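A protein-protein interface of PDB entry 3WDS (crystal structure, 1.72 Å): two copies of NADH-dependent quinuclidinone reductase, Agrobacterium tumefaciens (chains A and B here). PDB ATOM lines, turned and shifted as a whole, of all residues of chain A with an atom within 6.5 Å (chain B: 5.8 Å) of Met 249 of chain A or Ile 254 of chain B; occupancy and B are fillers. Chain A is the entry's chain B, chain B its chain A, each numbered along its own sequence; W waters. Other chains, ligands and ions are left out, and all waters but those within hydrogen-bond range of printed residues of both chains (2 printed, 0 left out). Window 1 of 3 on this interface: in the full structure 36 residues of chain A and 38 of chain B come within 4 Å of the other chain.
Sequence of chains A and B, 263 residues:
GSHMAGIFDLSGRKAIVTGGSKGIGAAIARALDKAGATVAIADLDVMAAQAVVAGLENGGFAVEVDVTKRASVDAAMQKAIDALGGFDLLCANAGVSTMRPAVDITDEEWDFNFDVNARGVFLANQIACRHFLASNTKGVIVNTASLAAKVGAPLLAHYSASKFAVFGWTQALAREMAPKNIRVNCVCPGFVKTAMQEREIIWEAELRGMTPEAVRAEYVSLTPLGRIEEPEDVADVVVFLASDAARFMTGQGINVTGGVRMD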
ATOM      1  N   ARG A 183     -24.805 -14.165  26.960  1.00  0.00           N
ATOM      2  CA  ARG A 183     -24.957 -15.567  26.622  1.00  0.00           C
ATOM      3  C   ARG A 183     -25.933 -16.225  27.531  1.00  0.00           C
ATOM      4  O   ARG A 183     -26.042 -15.917  28.730  1.00  0.00           O
ATOM      5  CB  ARG A 183     -23.633 -16.379  26.726  1.00  0.00           C
ATOM      6  CG  ARG A 183     -22.620 -15.897  25.718  1.00  0.00           C
ATOM      7  CD  ARG A 183     -21.350 -16.789  25.600  1.00  0.00           C
ATOM      8  NE  ARG A 183     -20.608 -16.826  26.917  1.00  0.00           N
ATOM      9  CZ  ARG A 183     -20.636 -17.819  27.761  1.00  0.00           C
ATOM     10  NH1 ARG A 183     -19.891 -17.777  28.849  1.00  0.00           N
ATOM     11  NH2 ARG A 183     -21.373 -18.910  27.559  1.00  0.00           N
ATOM     12  N   VAL A 184     -26.652 -17.185  26.968  1.00  0.00           N
ATOM     13  CA  VAL A 184     -27.702 -17.889  27.708  1.00  0.00           C
ATOM     14  C   VAL A 184     -27.659 -19.366  27.321  1.00  0.00           C
ATOM     15  O   VAL A 184     -28.020 -19.742  26.176  1.00  0.00           O
ATOM     16  CB  VAL A 184     -29.108 -17.337  27.438  1.00  0.00           C
ATOM     17  CG1 VAL A 184     -30.131 -18.012  28.349  1.00  0.00           C
ATOM     18  CG2 VAL A 184     -29.146 -15.825  27.517  1.00  0.00           C
ATOM     19  N   ASN A 185     -27.354 -20.228  28.280  1.00  0.00           N
ATOM     20  CA  ASN A 185     -27.306 -21.671  28.025  1.00  0.00           C
ATOM     21  C   ASN A 185     -28.053 -22.415  29.106  1.00  0.00           C
ATOM     22  O   ASN A 185     -28.374 -21.834  30.159  1.00  0.00           O
ATOM     23  CB  ASN A 185     -25.852 -22.198  27.954  1.00  0.00           C
ATOM     24  CG  ASN A 185     -25.103 -21.706  26.760  1.00  0.00           C
ATOM     25  OD1 ASN A 185     -25.368 -22.117  25.641  1.00  0.00           O
ATOM     26  ND2 ASN A 185     -24.196 -20.777  26.976  1.00  0.00           N
ATOM     27  N   PHE A 240     -17.863 -24.221  33.595  1.00  0.00           N
ATOM     28  CA  PHE A 240     -17.475 -24.088  32.225  1.00  0.00           C
ATOM     29  C   PHE A 240     -18.380 -23.090  31.445  1.00  0.00           C
ATOM     30  O   PHE A 240     -17.902 -22.146  30.782  1.00  0.00           O
ATOM     31  CB  PHE A 240     -17.472 -25.466  31.581  1.00  0.00           C
ATOM     32  CG  PHE A 240     -17.427 -25.397  30.077  1.00  0.00           C
ATOM     33  CD1 PHE A 240     -16.316 -24.831  29.433  1.00  0.00           C
ATOM     34  CD2 PHE A 240     -18.492 -25.814  29.381  1.00  0.00           C
ATOM     35  CE1 PHE A 240     -16.275 -24.750  28.032  1.00  0.00           C
ATOM     36  CE2 PHE A 240     -18.511 -25.666  27.987  1.00  0.00           C
ATOM     37  CZ  PHE A 240     -17.376 -25.160  27.338  1.00  0.00           C
ATOM     38  N   LEU A 241     -19.687 -23.307  31.500  1.00  0.00           N
ATOM     39  CA  LEU A 241     -20.613 -22.490  30.693  1.00  0.00           C
ATOM     40  C   LEU A 241     -20.666 -21.033  31.128  1.00  0.00           C
ATOM     41  O   LEU A 241     -20.947 -20.117  30.352  1.00  0.00           O
ATOM     42  CB  LEU A 241     -22.024 -23.119  30.758  1.00  0.00           C
ATOM     43  CG  LEU A 241     -22.146 -24.443  30.004  1.00  0.00           C
ATOM     44  CD1 LEU A 241     -23.496 -25.095  30.261  1.00  0.00           C
ATOM     45  CD2 LEU A 241     -22.034 -24.210  28.520  1.00  0.00           C
ATOM     46  N   ALA A 245     -14.316 -19.722  28.610  1.00  0.00           N
ATOM     47  CA  ALA A 245     -14.017 -20.858  27.725  1.00  0.00           C
ATOM     48  C   ALA A 245     -15.224 -21.170  26.865  1.00  0.00           C
ATOM     49  O   ALA A 245     -15.067 -21.748  25.772  1.00  0.00           O
ATOM     50  CB  ALA A 245     -13.579 -22.092  28.500  1.00  0.00           C
ATOM     51  N   ALA A 246     -16.378 -20.780  27.328  1.00  0.00           N
ATOM     52  CA  ALA A 246     -17.602 -20.964  26.599  1.00  0.00           C
ATOM     53  C   ALA A 246     -18.087 -19.696  25.911  1.00  0.00           C
ATOM     54  O   ALA A 246     -19.285 -19.597  25.574  1.00  0.00           O
ATOM     55  CB  ALA A 246     -18.698 -21.599  27.493  1.00  0.00           C
ATOM     56  N   ARG A 247     -17.170 -18.762  25.630  1.00  0.00           N
ATOM     57  CA  ARG A 247     -17.501 -17.494  25.061  1.00  0.00           C
ATOM     58  C   ARG A 247     -18.181 -17.566  23.703  1.00  0.00           C
ATOM     59  O   ARG A 247     -18.859 -16.602  23.332  1.00  0.00           O
ATOM     60  CB  ARG A 247     -16.281 -16.594  24.948  1.00  0.00           C
ATOM     61  CG  ARG A 247     -15.249 -17.111  23.950  1.00  0.00           C
ATOM     62  CD  ARG A 247     -13.959 -16.374  24.148  1.00  0.00           C
ATOM     63  NE  ARG A 247     -12.877 -16.921  23.394  1.00  0.00           N
ATOM     64  CZ  ARG A 247     -12.133 -17.961  23.730  1.00  0.00           C
ATOM     65  NH1 ARG A 247     -12.314 -18.567  24.859  1.00  0.00           N
ATOM     66  NH2 ARG A 247     -11.165 -18.353  22.930  1.00  0.00           N
ATOM     67  N   PHE A 248     -18.037 -18.683  22.958  1.00  0.00           N
ATOM     68  CA  PHE A 248     -18.650 -18.754  21.634  1.00  0.00           C
ATOM     69  C   PHE A 248     -19.779 -19.780  21.621  1.00  0.00           C
ATOM     70  O   PHE A 248     -20.097 -20.353  20.577  1.00  0.00           O
ATOM     71  CB  PHE A 248     -17.642 -19.042  20.495  1.00  0.00           C
ATOM     72  CG  PHE A 248     -18.035 -18.373  19.201  1.00  0.00           C
ATOM     73  CD1 PHE A 248     -18.093 -16.996  19.119  1.00  0.00           C
ATOM     74  CD2 PHE A 248     -18.259 -19.116  18.087  1.00  0.00           C
ATOM     75  CE1 PHE A 248     -18.461 -16.348  17.926  1.00  0.00           C
ATOM     76  CE2 PHE A 248     -18.642 -18.513  16.918  1.00  0.00           C
ATOM     77  CZ  PHE A 248     -18.723 -17.147  16.833  1.00  0.00           C
ATOM     78  N   MET A 249     -20.392 -19.980  22.785  1.00  0.00           N
ATOM     79  CA  MET A 249     -21.504 -20.907  22.961  1.00  0.00           C
ATOM     80  C   MET A 249     -22.719 -20.247  23.568  1.00  0.00           C
ATOM     81  O   MET A 249     -22.675 -19.710  24.686  1.00  0.00           O
ATOM     82  CB  MET A 249     -21.123 -22.040  23.881  1.00  0.00           C
ATOM     83  CG  MET A 249     -19.988 -22.951  23.379  1.00  0.00           C
ATOM     84  SD  MET A 249     -19.570 -24.270  24.488  1.00  0.00           S
ATOM     85  CE  MET A 249     -21.121 -25.114  24.709  1.00  0.00           C
ATOM     86  N   THR A 250     -23.831 -20.302  22.861  1.00  0.00           N
ATOM     87  CA  THR A 250     -25.055 -19.788  23.414  1.00  0.00           C
ATOM     88  C   THR A 250     -26.302 -20.505  22.892  1.00  0.00           C
ATOM     89  O   THR A 250     -26.324 -21.006  21.758  1.00  0.00           O
ATOM     90  CB  THR A 250     -25.155 -18.256  23.198  1.00  0.00           C
ATOM     91  OG1 THR A 250     -26.183 -17.750  24.042  1.00  0.00           O
ATOM     92  CG2 THR A 250     -25.446 -17.912  21.800  1.00  0.00           C
ATOM     93  N   GLY A 251     -27.336 -20.603  23.753  1.00  0.00           N
ATOM     94  CA  GLY A 251     -28.551 -21.300  23.421  1.00  0.00           C
ATOM     95  C   GLY A 251     -28.566 -22.823  23.495  1.00  0.00           C
ATOM     96  O   GLY A 251     -29.508 -23.458  22.978  1.00  0.00           O
ATOM     97  N   GLN A 252     -27.513 -23.395  24.056  1.00  0.00           N
ATOM     98  CA  GLN A 252     -27.343 -24.837  24.144  1.00  0.00           C
ATOM     99  C   GLN A 252     -28.066 -25.448  25.342  1.00  0.00           C
ATOM    100  O   GLN A 252     -28.374 -24.763  26.312  1.00  0.00           O
ATOM    101  CB  GLN A 252     -25.860 -25.199  24.125  1.00  0.00           C
ATOM    102  CG  GLN A 252     -25.029 -24.553  23.076  1.00  0.00           C
ATOM    103  CD  GLN A 252     -25.537 -24.745  21.663  1.00  0.00           C
ATOM    104  OE1 GLN A 252     -25.742 -23.757  20.896  1.00  0.00           O
ATOM    105  NE2 GLN A 252     -25.777 -25.956  21.330  1.00  0.00           N
ATOM    106  N   ILE A 254     -26.804 -28.393  27.280  1.00  0.00           N
ATOM    107  CA  ILE A 254     -25.694 -29.284  27.374  1.00  0.00           C
ATOM    108  C   ILE A 254     -26.095 -30.452  28.240  1.00  0.00           C
ATOM    109  O   ILE A 254     -26.426 -30.229  29.415  1.00  0.00           O
ATOM    110  CB  ILE A 254     -24.460 -28.556  28.022  1.00  0.00           C
ATOM    111  CG1 ILE A 254     -24.009 -27.358  27.152  1.00  0.00           C
ATOM    112  CG2 ILE A 254     -23.341 -29.545  28.126  1.00  0.00           C
ATOM    113  CD1 ILE A 254     -23.671 -27.680  25.744  1.00  0.00           C
ATOM    114  N   ASN A 255     -26.027 -31.702  27.720  1.00  0.00           N
ATOM    115  CA  ASN A 255     -26.392 -32.899  28.484  1.00  0.00           C
ATOM    116  C   ASN A 255     -25.263 -33.229  29.454  1.00  0.00           C
ATOM    117  O   ASN A 255     -24.123 -33.276  29.050  1.00  0.00           O
ATOM    118  CB  ASN A 255     -26.606 -34.099  27.561  1.00  0.00           C
ATOM    119  CG  ASN A 255     -27.763 -33.912  26.651  1.00  0.00           C
ATOM    120  OD1 ASN A 255     -28.768 -33.270  27.034  1.00  0.00           O
ATOM    121  ND2 ASN A 255     -27.608 -34.342  25.379  1.00  0.00           N
ATOM    122  N   ASP A 263     -26.695 -35.397  22.281  1.00  0.00           N
ATOM    123  CA  ASP A 263     -27.064 -34.373  21.265  1.00  0.00           C
ATOM    124  C   ASP A 263     -25.890 -33.503  20.709  1.00  0.00           C
ATOM    125  O   ASP A 263     -24.847 -33.654  21.528  1.00  0.00           O
ATOM    126  CB  ASP A 263     -28.060 -33.370  21.857  1.00  0.00           C
ATOM    127  CG  ASP A 263     -29.384 -34.000  22.226  1.00  0.00           C
ATOM    128  OD1 ASP A 263     -30.119 -34.423  21.286  1.00  0.00           O
ATOM    129  OD2 ASP A 263     -29.765 -34.037  23.425  1.00  0.00           O
ATOM    130  N   LYS B 150     -24.620 -31.537  12.103  1.00  0.00           N
ATOM    131  CA  LYS B 150     -25.917 -31.233  12.696  1.00  0.00           C
ATOM    132  C   LYS B 150     -26.929 -30.773  11.691  1.00  0.00           C
ATOM    133  O   LYS B 150     -28.149 -31.088  11.864  1.00  0.00           O
ATOM    134  CB  LYS B 150     -25.833 -30.156  13.754  1.00  0.00           C
ATOM    135  CG  LYS B 150     -24.857 -30.488  14.943  1.00  0.00           C
ATOM    136  CD  LYS B 150     -25.352 -31.689  15.777  1.00  0.00           C
ATOM    137  CE  LYS B 150     -24.568 -31.936  17.041  1.00  0.00           C
ATOM    138  NZ  LYS B 150     -24.876 -30.914  18.050  1.00  0.00           N
ATOM    139  N   ASN B 185     -16.264 -37.719  22.921  1.00  0.00           N
ATOM    140  CA  ASN B 185     -17.167 -36.636  22.547  1.00  0.00           C
ATOM    141  C   ASN B 185     -16.697 -36.013  21.287  1.00  0.00           C
ATOM    142  O   ASN B 185     -15.575 -36.267  20.839  1.00  0.00           O
ATOM    143  CB  ASN B 185     -17.253 -35.558  23.650  1.00  0.00           C
ATOM    144  CG  ASN B 185     -17.934 -36.040  24.910  1.00  0.00           C
ATOM    145  OD1 ASN B 185     -19.155 -36.202  24.984  1.00  0.00           O
ATOM    146  ND2 ASN B 185     -17.112 -36.321  25.942  1.00  0.00           N
ATOM    147  N   CYS B 186     -17.509 -35.162  20.672  1.00  0.00           N
ATOM    148  CA  CYS B 186     -17.036 -34.377  19.565  1.00  0.00           C
ATOM    149  C   CYS B 186     -17.489 -32.949  19.732  1.00  0.00           C
ATOM    150  O   CYS B 186     -18.413 -32.661  20.509  1.00  0.00           O
ATOM    151  CB  CYS B 186     -17.458 -34.970  18.176  1.00  0.00           C
ATOM    152  SG  CYS B 186     -19.235 -34.875  17.813  1.00  0.00           S
ATOM    153  N   VAL B 187     -16.798 -32.038  19.054  1.00  0.00           N
ATOM    154  CA  VAL B 187     -17.109 -30.590  18.976  1.00  0.00           C
ATOM    155  C   VAL B 187     -17.552 -30.271  17.537  1.00  0.00           C
ATOM    156  O   VAL B 187     -17.033 -30.857  16.571  1.00  0.00           O
ATOM    157  CB  VAL B 187     -15.963 -29.653  19.337  1.00  0.00           C
ATOM    158  CG1 VAL B 187     -15.752 -29.759  20.781  1.00  0.00           C
ATOM    159  CG2 VAL B 187     -14.699 -29.961  18.558  1.00  0.00           C
ATOM    160  N   CYS B 188     -18.553 -29.421  17.433  1.00  0.00           N
ATOM    161  CA  CYS B 188     -19.121 -29.029  16.154  1.00  0.00           C
ATOM    162  C   CYS B 188     -18.933 -27.530  15.935  1.00  0.00           C
ATOM    163  O   CYS B 188     -19.751 -26.730  16.333  1.00  0.00           O
ATOM    164  CB  CYS B 188     -20.606 -29.368  16.117  1.00  0.00           C
ATOM    165  SG  CYS B 188     -20.854 -31.163  16.246  1.00  0.00           S
ATOM    166  N   PRO B 189     -17.826 -27.136  15.319  1.00  0.00           N
ATOM    167  CA  PRO B 189     -17.552 -25.726  15.113  1.00  0.00           C
ATOM    168  C   PRO B 189     -18.412 -25.091  14.043  1.00  0.00           C
ATOM    169  O   PRO B 189     -18.855 -25.802  13.120  1.00  0.00           O
ATOM    170  CB  PRO B 189     -16.061 -25.679  14.669  1.00  0.00           C
ATOM    171  CG  PRO B 189     -15.546 -27.024  14.943  1.00  0.00           C
ATOM    172  CD  PRO B 189     -16.695 -27.998  14.964  1.00  0.00           C
ATOM    173  N   LEU B 225     -23.935 -14.345  17.847  1.00  0.00           N
ATOM    174  CA  LEU B 225     -22.948 -13.574  18.593  1.00  0.00           C
ATOM    175  C   LEU B 225     -22.207 -12.561  17.695  1.00  0.00           C
ATOM    176  O   LEU B 225     -21.397 -11.775  18.189  1.00  0.00           O
ATOM    177  CB  LEU B 225     -21.959 -14.478  19.368  1.00  0.00           C
ATOM    178  CG  LEU B 225     -22.454 -15.165  20.630  1.00  0.00           C
ATOM    179  CD1 LEU B 225     -21.477 -16.136  21.211  1.00  0.00           C
ATOM    180  CD2 LEU B 225     -22.777 -14.115  21.672  1.00  0.00           C
ATOM    181  N   VAL B 237     -13.030 -25.177  24.275  1.00  0.00           N
ATOM    182  CA  VAL B 237     -14.064 -26.137  24.563  1.00  0.00           C
ATOM    183  C   VAL B 237     -13.489 -27.542  24.509  1.00  0.00           C
ATOM    184  O   VAL B 237     -13.897 -28.434  25.317  1.00  0.00           O
ATOM    185  CB  VAL B 237     -15.263 -25.960  23.598  1.00  0.00           C
ATOM    186  CG1 VAL B 237     -16.330 -27.015  23.864  1.00  0.00           C
ATOM    187  CG2 VAL B 237     -15.760 -24.510  23.666  1.00  0.00           C
ATOM    188  N   LEU B 241     -13.694 -30.472  27.302  1.00  0.00           N
ATOM    189  CA  LEU B 241     -14.100 -31.846  27.105  1.00  0.00           C
ATOM    190  C   LEU B 241     -13.055 -32.895  27.464  1.00  0.00           C
ATOM    191  O   LEU B 241     -13.407 -34.006  27.814  1.00  0.00           O
ATOM    192  CB  LEU B 241     -14.572 -32.087  25.663  1.00  0.00           C
ATOM    193  CG  LEU B 241     -15.857 -31.346  25.316  1.00  0.00           C
ATOM    194  CD1 LEU B 241     -16.126 -31.409  23.819  1.00  0.00           C
ATOM    195  CD2 LEU B 241     -17.034 -31.991  26.035  1.00  0.00           C
ATOM    196  N   MET B 249     -19.829 -36.575  30.979  1.00  0.00           N
ATOM    197  CA  MET B 249     -20.308 -36.307  29.609  1.00  0.00           C
ATOM    198  C   MET B 249     -19.653 -37.239  28.607  1.00  0.00           C
ATOM    199  O   MET B 249     -18.411 -37.226  28.473  1.00  0.00           O
ATOM    200  CB  MET B 249     -19.978 -34.888  29.218  1.00  0.00           C
ATOM    201  CG  MET B 249     -20.625 -33.805  30.082  1.00  0.00           C
ATOM    202  SD  MET B 249     -20.210 -32.118  29.638  1.00  0.00           S
ATOM    203  CE  MET B 249     -20.740 -31.986  27.924  1.00  0.00           C
ATOM    204  N   GLN B 252     -21.369 -36.831  23.175  1.00  0.00           N
ATOM    205  CA  GLN B 252     -22.001 -35.519  22.799  1.00  0.00           C
ATOM    206  C   GLN B 252     -21.406 -34.918  21.529  1.00  0.00           C
ATOM    207  O   GLN B 252     -20.258 -35.201  21.159  1.00  0.00           O
ATOM    208  CB  GLN B 252     -21.935 -34.515  23.919  1.00  0.00           C
ATOM    209  CG  GLN B 252     -22.467 -34.985  25.261  1.00  0.00           C
ATOM    210  CD  GLN B 252     -23.867 -35.496  25.209  1.00  0.00           C
ATOM    211  OE1 GLN B 252     -24.781 -34.802  24.753  1.00  0.00           O
ATOM    212  NE2 GLN B 252     -24.054 -36.716  25.626  1.00  0.00           N
ATOM    213  N   GLY B 253     -22.192 -34.043  20.868  1.00  0.00           N
ATOM    214  CA  GLY B 253     -21.742 -33.172  19.767  1.00  0.00           C
ATOM    215  C   GLY B 253     -21.933 -31.763  20.277  1.00  0.00           C
ATOM    216  O   GLY B 253     -22.993 -31.139  20.052  1.00  0.00           O
ATOM    217  N   ILE B 254     -20.926 -31.250  20.953  1.00  0.00           N
ATOM    218  CA  ILE B 254     -20.997 -29.927  21.504  1.00  0.00           C
ATOM    219  C   ILE B 254     -20.848 -28.845  20.420  1.00  0.00           C
ATOM    220  O   ILE B 254     -19.799 -28.737  19.784  1.00  0.00           O
ATOM    221  CB  ILE B 254     -19.933 -29.747  22.621  1.00  0.00           C
ATOM    222  CG1 ILE B 254     -20.069 -30.763  23.738  1.00  0.00           C
ATOM    223  CG2 ILE B 254     -20.023 -28.316  23.183  1.00  0.00           C
ATOM    224  CD1 ILE B 254     -21.419 -30.789  24.460  1.00  0.00           C
ATOM    225  N   ASN B 255     -21.910 -28.057  20.233  1.00  0.00           N
ATOM    226  CA  ASN B 255     -21.882 -26.954  19.318  1.00  0.00           C
ATOM    227  C   ASN B 255     -21.026 -25.867  19.856  1.00  0.00           C
ATOM    228  O   ASN B 255     -21.245 -25.410  21.017  1.00  0.00           O
ATOM    229  CB  ASN B 255     -23.298 -26.439  19.005  1.00  0.00           C
ATOM    230  CG  ASN B 255     -24.183 -27.501  18.373  1.00  0.00           C
ATOM    231  OD1 ASN B 255     -23.751 -28.327  17.569  1.00  0.00           O
ATOM    232  ND2 ASN B 255     -25.396 -27.568  18.831  1.00  0.00           N
ATOM    233  N   VAL B 256     -20.164 -25.326  18.998  1.00  0.00           N
ATOM    234  CA  VAL B 256     -19.367 -24.156  19.301  1.00  0.00           C
ATOM    235  C   VAL B 256     -19.463 -23.294  18.064  1.00  0.00           C
ATOM    236  O   VAL B 256     -18.581 -23.284  17.212  1.00  0.00           O
ATOM    237  CB  VAL B 256     -17.914 -24.458  19.738  1.00  0.00           C
ATOM    238  CG1 VAL B 256     -17.296 -23.209  20.334  1.00  0.00           C
ATOM    239  CG2 VAL B 256     -17.837 -25.660  20.640  1.00  0.00           C
ATOM    240  N   THR B 257     -20.583 -22.561  17.961  1.00  0.00           N
ATOM    241  CA  THR B 257     -21.015 -21.933  16.688  1.00  0.00           C
ATOM    242  C   THR B 257     -21.468 -20.471  16.884  1.00  0.00           C
ATOM    243  O   THR B 257     -21.899 -19.820  15.914  1.00  0.00           O
ATOM    244  CB  THR B 257     -22.173 -22.698  15.989  1.00  0.00           C
ATOM    245  OG1 THR B 257     -23.377 -22.503  16.757  1.00  0.00           O
ATOM    246  CG2 THR B 257     -21.883 -24.194  15.855  1.00  0.00           C
ATOM    247  N   GLY B 258     -21.377 -19.929  18.110  1.00  0.00           N
ATOM    248  CA  GLY B 258     -21.859 -18.620  18.314  1.00  0.00           C
ATOM    249  C   GLY B 258     -23.390 -18.446  18.237  1.00  0.00           C
ATOM    250  O   GLY B 258     -23.853 -17.322  17.952  1.00  0.00           O
ATOM    251  N   GLY B 259     -24.123 -19.533  18.494  1.00  0.00           N
ATOM    252  CA  GLY B 259     -25.570 -19.585  18.486  1.00  0.00           C
ATOM    253  C   GLY B 259     -26.199 -19.986  17.169  1.00  0.00           C
ATOM    254  O   GLY B 259     -27.417 -19.945  17.014  1.00  0.00           O
HETATM  255  O   HOH W   1     -24.122 -28.023  22.210  1.00  0.00           O
HETATM  256  O   HOH W   2     -24.720 -32.038  25.203  1.00  0.00           O
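Ala 245 of chain A touches Val 237 of chain B (O to CG2, 3.5 Å). O of Arg 247 of chain A touches CD1 of Leu 225 of chain B, at 3.4 Å. CA of Phe 248 of chain A touches CD1 of Leu 225 of chain B (3.9 Å). Phe 248 of chain A touches Val 256 of chain B. CG2 of Val 237 of chain B touches SD of Met 249 of chain A (3.9 Å). Met 249 of chain A touches Asn 255 of chain B. Gly 259 of chain B touches Thr 250 of chain A. Met 249 of chain B touches Ile 254 of chain A (CE to CG2, 3.6 Å). CG of Met 249 of chain B touches O of Asn 255 of chain A, at 3.7 Å. Asp 263 of chain A touches Lys 150 of chain B.
The guanidinium group (NH2) of Arg 183 of chain A is in hydrogen-bond range of the backbone carbonyl oxygen (O) of Met 249 of chain A (3.3 Å). The side-chain amide nitrogen (ND2) of Asn 185 of chain B sits at hydrogen-bond distance from the backbone carbonyl oxygen (O) of Met 249 of chain B (3.0 Å). The backbone NH (N) of Leu 225 of chain B sits at hydrogen-bond distance from the backbone carbonyl oxygen (O) of Gly 258 of chain B (3.0 Å). The backbone carbonyl oxygen (O) of Cys 186 of chain B sits at hydrogen-bond distance from the backbone NH (N) of Ile 254 of chain B (2.9 Å). The side-chain amide nitrogen (ND2) of Asn 185 of chain A is in hydrogen-bond range of the backbone carbonyl oxygen (O) of Met 249 of chain A, at 2.9 Å. N of Gln 252 of chain A lies within hydrogen-bond range of OD1 of Asn 185 of chain A, 3.0 Å away.
Water W1 bridges NE2 of Gln 252 of chain A (2.8 Å) and N of Asn 255 of chain B (3.0 Å). Water W2 lies within hydrogen-bond range of OE1 of Gln 252 of chain B (2.8 Å) and N of Asn 255 of chain A (2.9 Å).
Printed residues of chain B within 4 Å of Ala 245 of chain A: Val 237. Met 249 of chain A touches three residues of chain B. Gly 251 of chain A touches none of the printed residues of chain B. Printed residues of chain B within 4 Å of Asp 263 of chain A: Lys 150 (3.8 Å), Gln 252 (3.2 Å) and Gly 253 (2.8 Å). Leu 241 of chain B touches none of the printed residues of chain A. Ile 254 of chain B touches just one residue of chain A: Met 249 (3.7 Å). Printed residues of chain A within 4 Å of Val 256 of chain B: Phe 248. Printed residues of chain A within 4 Å of Gly 258 of chain B: Phe 248 (2.8 Å). The nearest residue of chain B that does not touch Met 249 of chain A is Val 256 of chain B (4.1 Å). The nearest residue of chain A that does not touch Ile 254 of chain B is Ile 254 of chain A (4.05 Å).
Met 249 of chain A touches Ile 254 of chain B, and with the chains exchanged Ile 254 of chain A touches Met 249 of chain B. Met 249 of chain A touches Asn 255 of chain B, and with the chains exchanged Asn 255 of chain A touches Met 249 of chain B. Gln 252 of chain A touches Asn 255 of chain B, and with the chains exchanged Asn 255 of chain A touches Gln 252 of chain B. 6 positions are printed for both chains. Of the 17 pairs that touch across the chains among the printed residues, 6 have their exchanged pair printed and touching as well.
Of the 16 printed residues of chain A, 9 touch a printed residue of chain B. Hydrophobic or aromatic side chains of chain A within 4 Å of the printed part of chain B: Phe 248, Met 249 and Ile 254. Along chain A the printed residues that touch a printed residue of chain B span positions 245 to 263. Of the 18 printed residues of chain B, 12 touch a printed residue of chain A. Printed residues of chain B that touch a printed residue of chain A: Lys 150, Leu 225, Val 237, Met 249, Gln 252, Gly 253, Ile 254, Asn 255, Val 256, Thr 257, Gly 258 and Gly 259. Hydrophobic or aromatic side chains of chain B that line the printed part of chain A: Leu 225, Val 237, Met 249 and Ile 254. Among the printed residues, 17 pairs touch across the chains.
The backbone carbonyl oxygen (O) of Asp 263 of chain A sits at hydrogen-bond distance from the backbone NH (N) of Gly 253 of chain B (2.8 Å). The side-chain amide nitrogen (ND2) of Asn 255 of chain B lies close to the side-chain amide nitrogen (NE2) of Gln 252 of chain A (3.0 Å). N of Thr 257 of chain B is in hydrogen-bond range of O of Phe 248 of chain A, 3.5 Å away. The side-chain amide oxygen (OE1) of Gln 252 of chain B is in hydrogen-bond range of the backbone NH (N) of Asp 263 of chain A (3.2 Å). The backbone NH (N) of Gly 258 of chain B is in hydrogen-bond range of the backbone carbonyl oxygen (O) of Phe 248 of chain A (2.8 Å). The side-chain amide nitrogen of Asn 255 of chain A lies within hydrogen-bond range of the side-chain amide oxygen of Gln 252 of chain B (2.9 Å).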
